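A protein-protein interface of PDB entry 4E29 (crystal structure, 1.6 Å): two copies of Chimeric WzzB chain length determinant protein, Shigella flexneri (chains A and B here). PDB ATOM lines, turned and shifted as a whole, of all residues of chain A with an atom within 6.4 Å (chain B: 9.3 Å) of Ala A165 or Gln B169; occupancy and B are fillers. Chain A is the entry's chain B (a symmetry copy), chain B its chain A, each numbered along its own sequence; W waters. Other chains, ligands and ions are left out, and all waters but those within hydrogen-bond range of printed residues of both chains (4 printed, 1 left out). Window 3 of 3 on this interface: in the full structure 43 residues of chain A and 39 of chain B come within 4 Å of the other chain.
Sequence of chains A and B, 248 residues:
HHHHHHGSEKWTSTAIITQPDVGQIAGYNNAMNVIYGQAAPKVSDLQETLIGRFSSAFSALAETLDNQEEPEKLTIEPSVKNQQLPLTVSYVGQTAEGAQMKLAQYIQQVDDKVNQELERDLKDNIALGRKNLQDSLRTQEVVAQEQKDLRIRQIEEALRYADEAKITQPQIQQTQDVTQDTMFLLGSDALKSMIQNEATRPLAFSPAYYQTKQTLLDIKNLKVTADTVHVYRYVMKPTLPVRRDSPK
Water W1 lies within hydrogen-bond range of O of Ile B172 (2.6 Å) and NE2 of Gln A171 (2.9 Å). Water W2 bridges the side-chain carboxylate of Asp B189 (2.7 Å) and the side-chain carboxylate of Glu A164 (3.1 Å). Water W4 bridges OG of Ser B193 (2.7 Å) and OE1 of Glu A164 (3.1 Å). Water W3 lies within hydrogen-bond range of OH of Tyr A161 and O of Met B194.
NE2 of Gln B169 sits at hydrogen-bond distance from OD2 of Asp B189 (2.8 Å). The backbone carbonyl oxygen of Gln B169 sits at hydrogen-bond distance from the side-chain amide nitrogen of Gln B171, at 2.9 Å. O of Ala A162 lies within hydrogen-bond range of N of Ile A167, at 2.9 Å. The backbone carbonyl oxygen of Thr B168 is in hydrogen-bond range of the backbone NH of Asp B189 (3.0 Å).
Of the printed residues of chain B, Glu A164 touches Asp B189 (3.4 Å) and Ser B193 (3.8 Å). Of chain B, only Gln B169 (3.0 Å) and Asp B189 (3.8 Å) come within 4 Å of Ala A165. Gln B169 touches just one residue of chain A: Ala A165. Printed residues of chain A within 4 Å of Pro B170: Ile A167 (3.6 Å), Gln A171 (3.7 Å) and Phe A184 (3.99 Å). Of the printed residues of chain A, Leu B186 touches Phe A184 (3.8 Å). Of the printed residues of chain A, Asp B189 touches Glu A164 (3.4 Å) and Ala A165 (3.8 Å). Of the printed residues of chain A, Met B194 touches Tyr A161.
Positions printed for both chains: 162, 163, 165, 166, 167, 171 and 184. Of the 12 pairs that touch across the chains among the printed residues, none has its exchanged pair printed and touching as well.
NE2 of Gln B169 sits at hydrogen-bond distance from O of Ala A165.
Among the printed residues, pairs that only touch across the chains: Tyr A161 with Ser B193, Glu A164 with Asp B189, Phe A184 with Ala B190, Tyr A161 with Met B194, Ile A167 with Pro B170, Arg A160 with Ser B193, Gln A171 with Pro B170, Phe A184 with Leu B186, Glu A164 with Ser B193, Ala A165 with Asp B189 and Phe A184 with Pro B170.
Of the 10 printed residues of chain A, 7 touch a printed residue of chain B. Of the 22 printed residues of chain B, 7 touch a printed residue of chain A. Hydrophobic or aromatic side chains of chain B that line the printed part of chain A: Pro B170, Ala B190 and Met B194. Among the printed residues, 12 pairs touch across the chains. Among the printed residues, no Asp or Glu carboxylate lies within 4 Å of a Lys or Arg side-chain nitrogen of the other chain.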
ATOM      1  N   ARG A 160      19.071 -19.148  -5.358  1.00  0.00           N
ATOM      2  CA  ARG A 160      17.698 -19.189  -5.857  1.00  0.00           C
ATOM      3  C   ARG A 160      17.556 -20.212  -6.963  1.00  0.00           C
ATOM      4  O   ARG A 160      16.573 -20.958  -7.015  1.00  0.00           O
ATOM      5  CB  ARG A 160      17.276 -17.833  -6.420  1.00  0.00           C
ATOM      6  CG  ARG A 160      17.391 -16.686  -5.473  1.00  0.00           C
ATOM      7  CD  ARG A 160      16.662 -15.462  -6.048  1.00  0.00           C
ATOM      8  NE  ARG A 160      17.253 -14.232  -5.556  1.00  0.00           N
ATOM      9  CZ  ARG A 160      17.047 -13.737  -4.341  1.00  0.00           C
ATOM     10  NH1 ARG A 160      16.239 -14.367  -3.493  1.00  0.00           N
ATOM     11  NH2 ARG A 160      17.650 -12.614  -3.978  1.00  0.00           N
ATOM     12  N   TYR A 161      18.518 -20.232  -7.880  1.00  0.00           N
ATOM     13  CA  TYR A 161      18.419 -21.127  -9.022  1.00  0.00           C
ATOM     14  C   TYR A 161      18.550 -22.581  -8.571  1.00  0.00           C
ATOM     15  O   TYR A 161      17.828 -23.462  -9.050  1.00  0.00           O
ATOM     16  CB  TYR A 161      19.503 -20.817 -10.057  1.00  0.00           C
ATOM     17  CG  TYR A 161      19.706 -19.342 -10.401  1.00  0.00           C
ATOM     18  CD1 TYR A 161      18.675 -18.406 -10.291  1.00  0.00           C
ATOM     19  CD2 TYR A 161      20.939 -18.898 -10.858  1.00  0.00           C
ATOM     20  CE1 TYR A 161      18.900 -17.052 -10.619  1.00  0.00           C
ATOM     21  CE2 TYR A 161      21.171 -17.564 -11.185  1.00  0.00           C
ATOM     22  CZ  TYR A 161      20.150 -16.646 -11.067  1.00  0.00           C
ATOM     23  OH  TYR A 161      20.425 -15.337 -11.404  1.00  0.00           O
ATOM     24  N   ALA A 162      19.473 -22.825  -7.640  1.00  0.00           N
ATOM     25  CA  ALA A 162      19.663 -24.176  -7.121  1.00  0.00           C
ATOM     26  C   ALA A 162      18.413 -24.641  -6.384  1.00  0.00           C
ATOM     27  O   ALA A 162      18.028 -25.801  -6.495  1.00  0.00           O
ATOM     28  CB  ALA A 162      20.880 -24.220  -6.205  1.00  0.00           C
ATOM     29  N   ASP A 163      17.765 -23.746  -5.643  1.00  0.00           N
ATOM     30  CA  ASP A 163      16.536 -24.127  -4.950  1.00  0.00           C
ATOM     31  C   ASP A 163      15.448 -24.497  -5.947  1.00  0.00           C
ATOM     32  O   ASP A 163      14.721 -25.474  -5.756  1.00  0.00           O
ATOM     33  CB  ASP A 163      16.059 -23.011  -4.023  1.00  0.00           C
ATOM     34  CG  ASP A 163      16.815 -22.982  -2.701  1.00  0.00           C
ATOM     35  OD1 ASP A 163      17.508 -23.977  -2.366  1.00  0.00           O
ATOM     36  OD2 ASP A 163      16.703 -21.967  -1.980  1.00  0.00           O
ATOM     37  N   GLU A 164      15.340 -23.729  -7.023  1.00  0.00           N
ATOM     38  CA  GLU A 164      14.330 -24.011  -8.036  1.00  0.00           C
ATOM     39  C   GLU A 164      14.573 -25.343  -8.729  1.00  0.00           C
ATOM     40  O   GLU A 164      13.622 -26.043  -9.108  1.00  0.00           O
ATOM     41  CB  GLU A 164      14.267 -22.873  -9.063  1.00  0.00           C
ATOM     42  CG  GLU A 164      13.107 -22.987 -10.040  1.00  0.00           C
ATOM     43  CD  GLU A 164      11.759 -22.764  -9.368  1.00  0.00           C
ATOM     44  OE1 GLU A 164      11.695 -22.040  -8.351  1.00  0.00           O
ATOM     45  OE2 GLU A 164      10.759 -23.326  -9.857  1.00  0.00           O
ATOM     46  N   ALA A 165      15.839 -25.711  -8.896  1.00  0.00           N
ATOM     47  CA  ALA A 165      16.164 -26.969  -9.558  1.00  0.00           C
ATOM     48  C   ALA A 165      16.261 -28.104  -8.528  1.00  0.00           C
ATOM     49  O   ALA A 165      16.442 -29.267  -8.895  1.00  0.00           O
ATOM     50  CB  ALA A 165      17.452 -26.831 -10.351  1.00  0.00           C
ATOM     51  N   LYS A 166      16.116 -27.741  -7.258  1.00  0.00           N
ATOM     52  CA  LYS A 166      16.263 -28.673  -6.140  1.00  0.00           C
ATOM     53  C   LYS A 166      17.608 -29.394  -6.160  1.00  0.00           C
ATOM     54  O   LYS A 166      17.692 -30.607  -5.956  1.00  0.00           O
ATOM     55  CB  LYS A 166      15.086 -29.653  -6.086  1.00  0.00           C
ATOM     56  CG  LYS A 166      13.816 -28.994  -5.559  1.00  0.00           C
ATOM     57  CD  LYS A 166      12.721 -30.023  -5.304  1.00  0.00           C
ATOM     58  CE  LYS A 166      12.125 -29.800  -3.937  1.00  0.00           C
ATOM     59  NZ  LYS A 166      11.727 -28.384  -3.758  1.00  0.00           N
ATOM     60  N   ILE A 167      18.670 -28.627  -6.397  1.00  0.00           N
ATOM     61  CA  ILE A 167      20.021 -29.156  -6.348  1.00  0.00           C
ATOM     62  C   ILE A 167      20.632 -28.754  -5.016  1.00  0.00           C
ATOM     63  O   ILE A 167      20.946 -27.578  -4.789  1.00  0.00           O
ATOM     64  CB  ILE A 167      20.847 -28.586  -7.514  1.00  0.00           C
ATOM     65  CG1 ILE A 167      20.189 -28.963  -8.849  1.00  0.00           C
ATOM     66  CG2 ILE A 167      22.289 -29.064  -7.462  1.00  0.00           C
ATOM     67  CD1 ILE A 167      20.891 -28.399 -10.036  1.00  0.00           C
ATOM     68  N   GLN A 171      26.771 -30.955  -8.325  1.00  0.00           N
ATOM     69  CA  GLN A 171      26.469 -31.800  -9.475  1.00  0.00           C
ATOM     70  C   GLN A 171      27.617 -31.865 -10.453  1.00  0.00           C
ATOM     71  O   GLN A 171      27.397 -31.940 -11.665  1.00  0.00           O
ATOM     72  CB  GLN A 171      25.236 -31.275 -10.215  1.00  0.00           C
ATOM     73  CG  GLN A 171      23.968 -31.386  -9.405  1.00  0.00           C
ATOM     74  CD  GLN A 171      22.865 -32.139 -10.130  1.00  0.00           C
ATOM     75  NE2 GLN A 171      22.743 -31.896 -11.430  1.00  0.00           N
ATOM     76  N   PHE A 184      25.139 -22.435  -9.491  1.00  0.00           N
ATOM     77  CA  PHE A 184      24.089 -23.253  -8.881  1.00  0.00           C
ATOM     78  C   PHE A 184      24.415 -24.739  -8.837  1.00  0.00           C
ATOM     79  O   PHE A 184      23.861 -25.492  -8.040  1.00  0.00           O
ATOM     80  CB  PHE A 184      22.723 -22.999  -9.541  1.00  0.00           C
ATOM     81  CG  PHE A 184      22.482 -23.752 -10.836  1.00  0.00           C
ATOM     82  CD1 PHE A 184      21.513 -24.750 -10.897  1.00  0.00           C
ATOM     83  CD2 PHE A 184      23.145 -23.391 -12.002  1.00  0.00           C
ATOM     84  CE1 PHE A 184      21.244 -25.425 -12.105  1.00  0.00           C
ATOM     85  CE2 PHE A 184      22.882 -24.055 -13.199  1.00  0.00           C
ATOM     86  CZ  PHE A 184      21.934 -25.062 -13.246  1.00  0.00           C
ATOM     87  N   ALA B 162      15.266 -25.557 -24.310  1.00  0.00           N
ATOM     88  CA  ALA B 162      15.248 -26.562 -23.260  1.00  0.00           C
ATOM     89  C   ALA B 162      13.853 -27.142 -23.165  1.00  0.00           C
ATOM     90  O   ALA B 162      13.688 -28.343 -22.957  1.00  0.00           O
ATOM     91  CB  ALA B 162      15.663 -25.962 -21.922  1.00  0.00           C
ATOM     92  N   ASP B 163      12.851 -26.289 -23.313  1.00  0.00           N
ATOM     93  CA  ASP B 163      11.474 -26.771 -23.263  1.00  0.00           C
ATOM     94  C   ASP B 163      11.193 -27.750 -24.401  1.00  0.00           C
ATOM     95  O   ASP B 163      10.476 -28.739 -24.218  1.00  0.00           O
ATOM     96  CB  ASP B 163      10.485 -25.608 -23.301  1.00  0.00           C
ATOM     97  CG  ASP B 163      10.273 -24.976 -21.937  1.00  0.00           C
ATOM     98  OD1 ASP B 163      10.670 -25.587 -20.916  1.00  0.00           O
ATOM     99  OD2 ASP B 163       9.693 -23.874 -21.883  1.00  0.00           O
ATOM    100  N   ALA B 165      13.373 -29.739 -25.877  1.00  0.00           N
ATOM    101  CA  ALA B 165      14.117 -30.975 -25.679  1.00  0.00           C
ATOM    102  C   ALA B 165      13.662 -31.649 -24.384  1.00  0.00           C
ATOM    103  O   ALA B 165      14.171 -32.709 -24.027  1.00  0.00           O
ATOM    104  CB  ALA B 165      15.607 -30.697 -25.637  1.00  0.00           C
ATOM    105  N   LYS B 166      12.718 -31.011 -23.693  1.00  0.00           N
ATOM    106  CA  LYS B 166      12.268 -31.465 -22.371  1.00  0.00           C
ATOM    107  C   LYS B 166      13.427 -31.702 -21.414  1.00  0.00           C
ATOM    108  O   LYS B 166      13.541 -32.755 -20.786  1.00  0.00           O
ATOM    109  CB  LYS B 166      11.357 -32.690 -22.508  1.00  0.00           C
ATOM    110  CG  LYS B 166      10.021 -32.304 -23.126  1.00  0.00           C
ATOM    111  CD  LYS B 166       9.039 -33.467 -23.158  1.00  0.00           C
ATOM    112  CE  LYS B 166       7.698 -32.999 -23.667  1.00  0.00           C
ATOM    113  NZ  LYS B 166       7.041 -32.095 -22.700  1.00  0.00           N
ATOM    114  N   ILE B 167      14.305 -30.705 -21.325  1.00  0.00           N
ATOM    115  CA  ILE B 167      15.432 -30.744 -20.409  1.00  0.00           C
ATOM    116  C   ILE B 167      15.096 -29.801 -19.247  1.00  0.00           C
ATOM    117  O   ILE B 167      15.087 -28.578 -19.427  1.00  0.00           O
ATOM    118  CB  ILE B 167      16.724 -30.299 -21.133  1.00  0.00           C
ATOM    119  CG1 ILE B 167      17.025 -31.256 -22.293  1.00  0.00           C
ATOM    120  CG2 ILE B 167      17.903 -30.240 -20.166  1.00  0.00           C
ATOM    121  CD1 ILE B 167      18.319 -30.967 -23.002  1.00  0.00           C
ATOM    122  N   THR B 168      14.769 -30.359 -18.083  1.00  0.00           N
ATOM    123  CA  THR B 168      14.396 -29.520 -16.928  1.00  0.00           C
ATOM    124  C   THR B 168      15.555 -29.375 -15.947  1.00  0.00           C
ATOM    125  O   THR B 168      15.672 -28.372 -15.251  1.00  0.00           O
ATOM    126  CB  THR B 168      13.154 -30.052 -16.201  1.00  0.00           C
ATOM    127  OG1 THR B 168      13.417 -31.362 -15.681  1.00  0.00           O
ATOM    128  CG2 THR B 168      11.988 -30.130 -17.171  1.00  0.00           C
ATOM    129  N   GLN B 169      16.420 -30.380 -15.928  1.00  0.00           N
ATOM    130  CA  GLN B 169      17.563 -30.415 -15.032  1.00  0.00           C
ATOM    131  C   GLN B 169      18.850 -30.226 -15.808  1.00  0.00           C
ATOM    132  O   GLN B 169      18.903 -30.475 -17.012  1.00  0.00           O
ATOM    133  CB  GLN B 169      17.584 -31.747 -14.305  1.00  0.00           C
ATOM    134  CG  GLN B 169      16.456 -31.848 -13.320  1.00  0.00           C
ATOM    135  CD  GLN B 169      16.777 -31.093 -12.056  1.00  0.00           C
ATOM    136  OE1 GLN B 169      17.796 -31.368 -11.419  1.00  0.00           O
ATOM    137  NE2 GLN B 169      15.936 -30.119 -11.694  1.00  0.00           N
ATOM    138  N   PRO B 170      19.906 -29.781 -15.122  1.00  0.00           N
ATOM    139  CA  PRO B 170      21.131 -29.502 -15.883  1.00  0.00           C
ATOM    140  C   PRO B 170      21.757 -30.782 -16.412  1.00  0.00           C
ATOM    141  O   PRO B 170      21.693 -31.817 -15.741  1.00  0.00           O
ATOM    142  CB  PRO B 170      22.059 -28.837 -14.856  1.00  0.00           C
ATOM    143  CG  PRO B 170      21.481 -29.149 -13.522  1.00  0.00           C
ATOM    144  CD  PRO B 170      20.002 -29.358 -13.715  1.00  0.00           C
ATOM    145  N   GLN B 171      22.359 -30.685 -17.598  1.00  0.00           N
ATOM    146  CA  GLN B 171      22.952 -31.829 -18.281  1.00  0.00           C
ATOM    147  C   GLN B 171      24.469 -31.754 -18.270  1.00  0.00           C
ATOM    148  O   GLN B 171      25.140 -32.669 -18.736  1.00  0.00           O
ATOM    149  CB  GLN B 171      22.473 -31.875 -19.736  1.00  0.00           C
ATOM    150  CG  GLN B 171      20.963 -31.957 -19.876  1.00  0.00           C
ATOM    151  CD  GLN B 171      20.401 -33.190 -19.202  1.00  0.00           C
ATOM    152  OE1 GLN B 171      20.780 -34.315 -19.534  1.00  0.00           O
ATOM    153  NE2 GLN B 171      19.505 -32.987 -18.235  1.00  0.00           N
ATOM    154  N   ILE B 172      25.014 -30.652 -17.777  1.00  0.00           N
ATOM    155  CA  ILE B 172      26.466 -30.528 -17.702  1.00  0.00           C
ATOM    156  C   ILE B 172      26.968 -30.835 -16.299  1.00  0.00           C
ATOM    157  O   ILE B 172      26.290 -30.553 -15.306  1.00  0.00           O
ATOM    158  CB  ILE B 172      26.957 -29.141 -18.128  1.00  0.00           C
ATOM    159  CG1 ILE B 172      26.304 -28.059 -17.275  1.00  0.00           C
ATOM    160  CG2 ILE B 172      26.676 -28.901 -19.616  1.00  0.00           C
ATOM    161  CD1 ILE B 172      26.946 -26.697 -17.461  1.00  0.00           C
ATOM    162  N   MET B 183      23.451 -22.755 -23.403  1.00  0.00           N
ATOM    163  CA  MET B 183      22.662 -22.332 -22.232  1.00  0.00           C
ATOM    164  C   MET B 183      21.526 -23.327 -21.926  1.00  0.00           C
ATOM    165  O   MET B 183      21.218 -23.578 -20.759  1.00  0.00           O
ATOM    166  CB  MET B 183      22.114 -20.898 -22.411  1.00  0.00           C
ATOM    167  N   PHE B 184      20.912 -23.901 -22.958  1.00  0.00           N
ATOM    168  CA  PHE B 184      19.784 -24.817 -22.715  1.00  0.00           C
ATOM    169  C   PHE B 184      20.157 -26.021 -21.860  1.00  0.00           C
ATOM    170  O   PHE B 184      19.311 -26.604 -21.194  1.00  0.00           O
ATOM    171  CB  PHE B 184      19.094 -25.258 -24.025  1.00  0.00           C
ATOM    172  CG  PHE B 184      19.746 -26.441 -24.729  1.00  0.00           C
ATOM    173  CD1 PHE B 184      19.159 -27.699 -24.697  1.00  0.00           C
ATOM    174  CD2 PHE B 184      20.919 -26.277 -25.447  1.00  0.00           C
ATOM    175  CE1 PHE B 184      19.741 -28.780 -25.346  1.00  0.00           C
ATOM    176  CE2 PHE B 184      21.511 -27.358 -26.103  1.00  0.00           C
ATOM    177  CZ  PHE B 184      20.924 -28.600 -26.054  1.00  0.00           C
ATOM    178  N   LEU B 185      21.437 -26.372 -21.857  1.00  0.00           N
ATOM    179  CA  LEU B 185      21.916 -27.505 -21.078  1.00  0.00           C
ATOM    180  C   LEU B 185      21.838 -27.262 -19.565  1.00  0.00           C
ATOM    181  O   LEU B 185      22.030 -28.180 -18.782  1.00  0.00           O
ATOM    182  CB  LEU B 185      23.351 -27.867 -21.497  1.00  0.00           C
ATOM    183  CG  LEU B 185      23.538 -28.297 -22.954  1.00  0.00           C
ATOM    184  CD1 LEU B 185      25.021 -28.269 -23.318  1.00  0.00           C
ATOM    185  CD2 LEU B 185      22.926 -29.679 -23.167  1.00  0.00           C
ATOM    186  N   LEU B 186      21.552 -26.034 -19.149  1.00  0.00           N
ATOM    187  CA  LEU B 186      21.392 -25.777 -17.722  1.00  0.00           C
ATOM    188  C   LEU B 186      20.037 -26.266 -17.237  1.00  0.00           C
ATOM    189  O   LEU B 186      19.852 -26.473 -16.045  1.00  0.00           O
ATOM    190  CB  LEU B 186      21.555 -24.290 -17.407  1.00  0.00           C
ATOM    191  CG  LEU B 186      22.897 -23.677 -17.845  1.00  0.00           C
ATOM    192  CD1 LEU B 186      22.914 -22.204 -17.490  1.00  0.00           C
ATOM    193  CD2 LEU B 186      24.045 -24.398 -17.174  1.00  0.00           C
ATOM    194  N   GLY B 187      19.106 -26.447 -18.171  1.00  0.00           N
ATOM    195  CA  GLY B 187      17.802 -27.002 -17.858  1.00  0.00           C
ATOM    196  C   GLY B 187      16.790 -25.913 -17.540  1.00  0.00           C
ATOM    197  O   GLY B 187      17.135 -24.854 -17.005  1.00  0.00           O
ATOM    198  N   SER B 188      15.528 -26.185 -17.847  1.00  0.00           N
ATOM    199  CA  SER B 188      14.486 -25.182 -17.709  1.00  0.00           C
ATOM    200  C   SER B 188      14.196 -24.759 -16.268  1.00  0.00           C
ATOM    201  O   SER B 188      13.785 -23.622 -16.029  1.00  0.00           O
ATOM    202  CB  SER B 188      13.208 -25.628 -18.424  1.00  0.00           C
ATOM    203  OG  SER B 188      12.694 -26.827 -17.866  1.00  0.00           O
ATOM    204  N   ASP B 189      14.408 -25.638 -15.291  1.00  0.00           N
ATOM    205  CA  ASP B 189      14.186 -25.189 -13.912  1.00  0.00           C
ATOM    206  C   ASP B 189      15.084 -23.979 -13.586  1.00  0.00           C
ATOM    207  O   ASP B 189      14.602 -22.941 -13.108  1.00  0.00           O
ATOM    208  CB  ASP B 189      14.440 -26.301 -12.910  1.00  0.00           C
ATOM    209  CG  ASP B 189      13.408 -27.427 -12.978  1.00  0.00           C
ATOM    210  OD1 ASP B 189      12.272 -27.217 -13.461  1.00  0.00           O
ATOM    211  OD2 ASP B 189      13.749 -28.535 -12.531  1.00  0.00           O
ATOM    212  N   ALA B 190      16.383 -24.109 -13.855  1.00  0.00           N
ATOM    213  CA  ALA B 190      17.321 -23.022 -13.564  1.00  0.00           C
ATOM    214  C   ALA B 190      17.087 -21.831 -14.469  1.00  0.00           C
ATOM    215  O   ALA B 190      17.097 -20.696 -14.003  1.00  0.00           O
ATOM    216  CB  ALA B 190      18.768 -23.511 -13.707  1.00  0.00           C
ATOM    217  N   LEU B 191      16.887 -22.089 -15.764  1.00  0.00           N
ATOM    218  CA  LEU B 191      16.712 -21.004 -16.720  1.00  0.00           C
ATOM    219  C   LEU B 191      15.504 -20.144 -16.350  1.00  0.00           C
ATOM    220  O   LEU B 191      15.581 -18.905 -16.378  1.00  0.00           O
ATOM    221  CB  LEU B 191      16.579 -21.543 -18.156  1.00  0.00           C
ATOM    222  CG  LEU B 191      17.832 -22.243 -18.703  1.00  0.00           C
ATOM    223  CD1 LEU B 191      17.485 -23.053 -19.928  1.00  0.00           C
ATOM    224  CD2 LEU B 191      18.956 -21.226 -19.020  1.00  0.00           C
ATOM    225  N   LYS B 192      14.401 -20.795 -15.978  1.00  0.00           N
ATOM    226  CA  LYS B 192      13.209 -20.049 -15.554  1.00  0.00           C
ATOM    227  C   LYS B 192      13.517 -19.167 -14.355  1.00  0.00           C
ATOM    228  O   LYS B 192      13.083 -18.021 -14.297  1.00  0.00           O
ATOM    229  CB  LYS B 192      12.086 -21.016 -15.178  1.00  0.00           C
ATOM    230  CG  LYS B 192      11.421 -21.666 -16.355  1.00  0.00           C
ATOM    231  CD  LYS B 192      10.482 -22.771 -15.864  1.00  0.00           C
ATOM    232  CE  LYS B 192       9.767 -23.459 -17.006  1.00  0.00           C
ATOM    233  NZ  LYS B 192       8.881 -24.539 -16.484  1.00  0.00           N
ATOM    234  N   SER B 193      14.276 -19.704 -13.400  1.00  0.00           N
ATOM    235  CA  SER B 193      14.616 -18.941 -12.205  1.00  0.00           C
ATOM    236  C   SER B 193      15.514 -17.737 -12.530  1.00  0.00           C
ATOM    237  O   SER B 193      15.330 -16.648 -11.983  1.00  0.00           O
ATOM    238  CB  SER B 193      15.273 -19.844 -11.163  1.00  0.00           C
ATOM    239  OG  SER B 193      15.420 -19.153  -9.941  1.00  0.00           O
ATOM    240  N   MET B 194      16.458 -17.934 -13.443  1.00  0.00           N
ATOM    241  CA  MET B 194      17.339 -16.845 -13.884  1.00  0.00           C
ATOM    242  C   MET B 194      16.550 -15.709 -14.535  1.00  0.00           C
ATOM    243  O   MET B 194      16.881 -14.524 -14.374  1.00  0.00           O
ATOM    244  CB  MET B 194      18.410 -17.416 -14.825  1.00  0.00           C
ATOM    245  CG  MET B 194      19.257 -18.328 -14.041  1.00  0.00           C
HETATM  246  O   HOH W   1      24.895 -31.456 -13.250  1.00  0.00           O
HETATM  247  O   HOH W   2      10.656 -25.348 -12.263  1.00  0.00           O
HETATM  248  O   HOH W   3      19.706 -14.225 -13.883  1.00  0.00           O
HETATM  249  O   HOH W   4      12.836 -19.178  -9.003  1.00  0.00           O
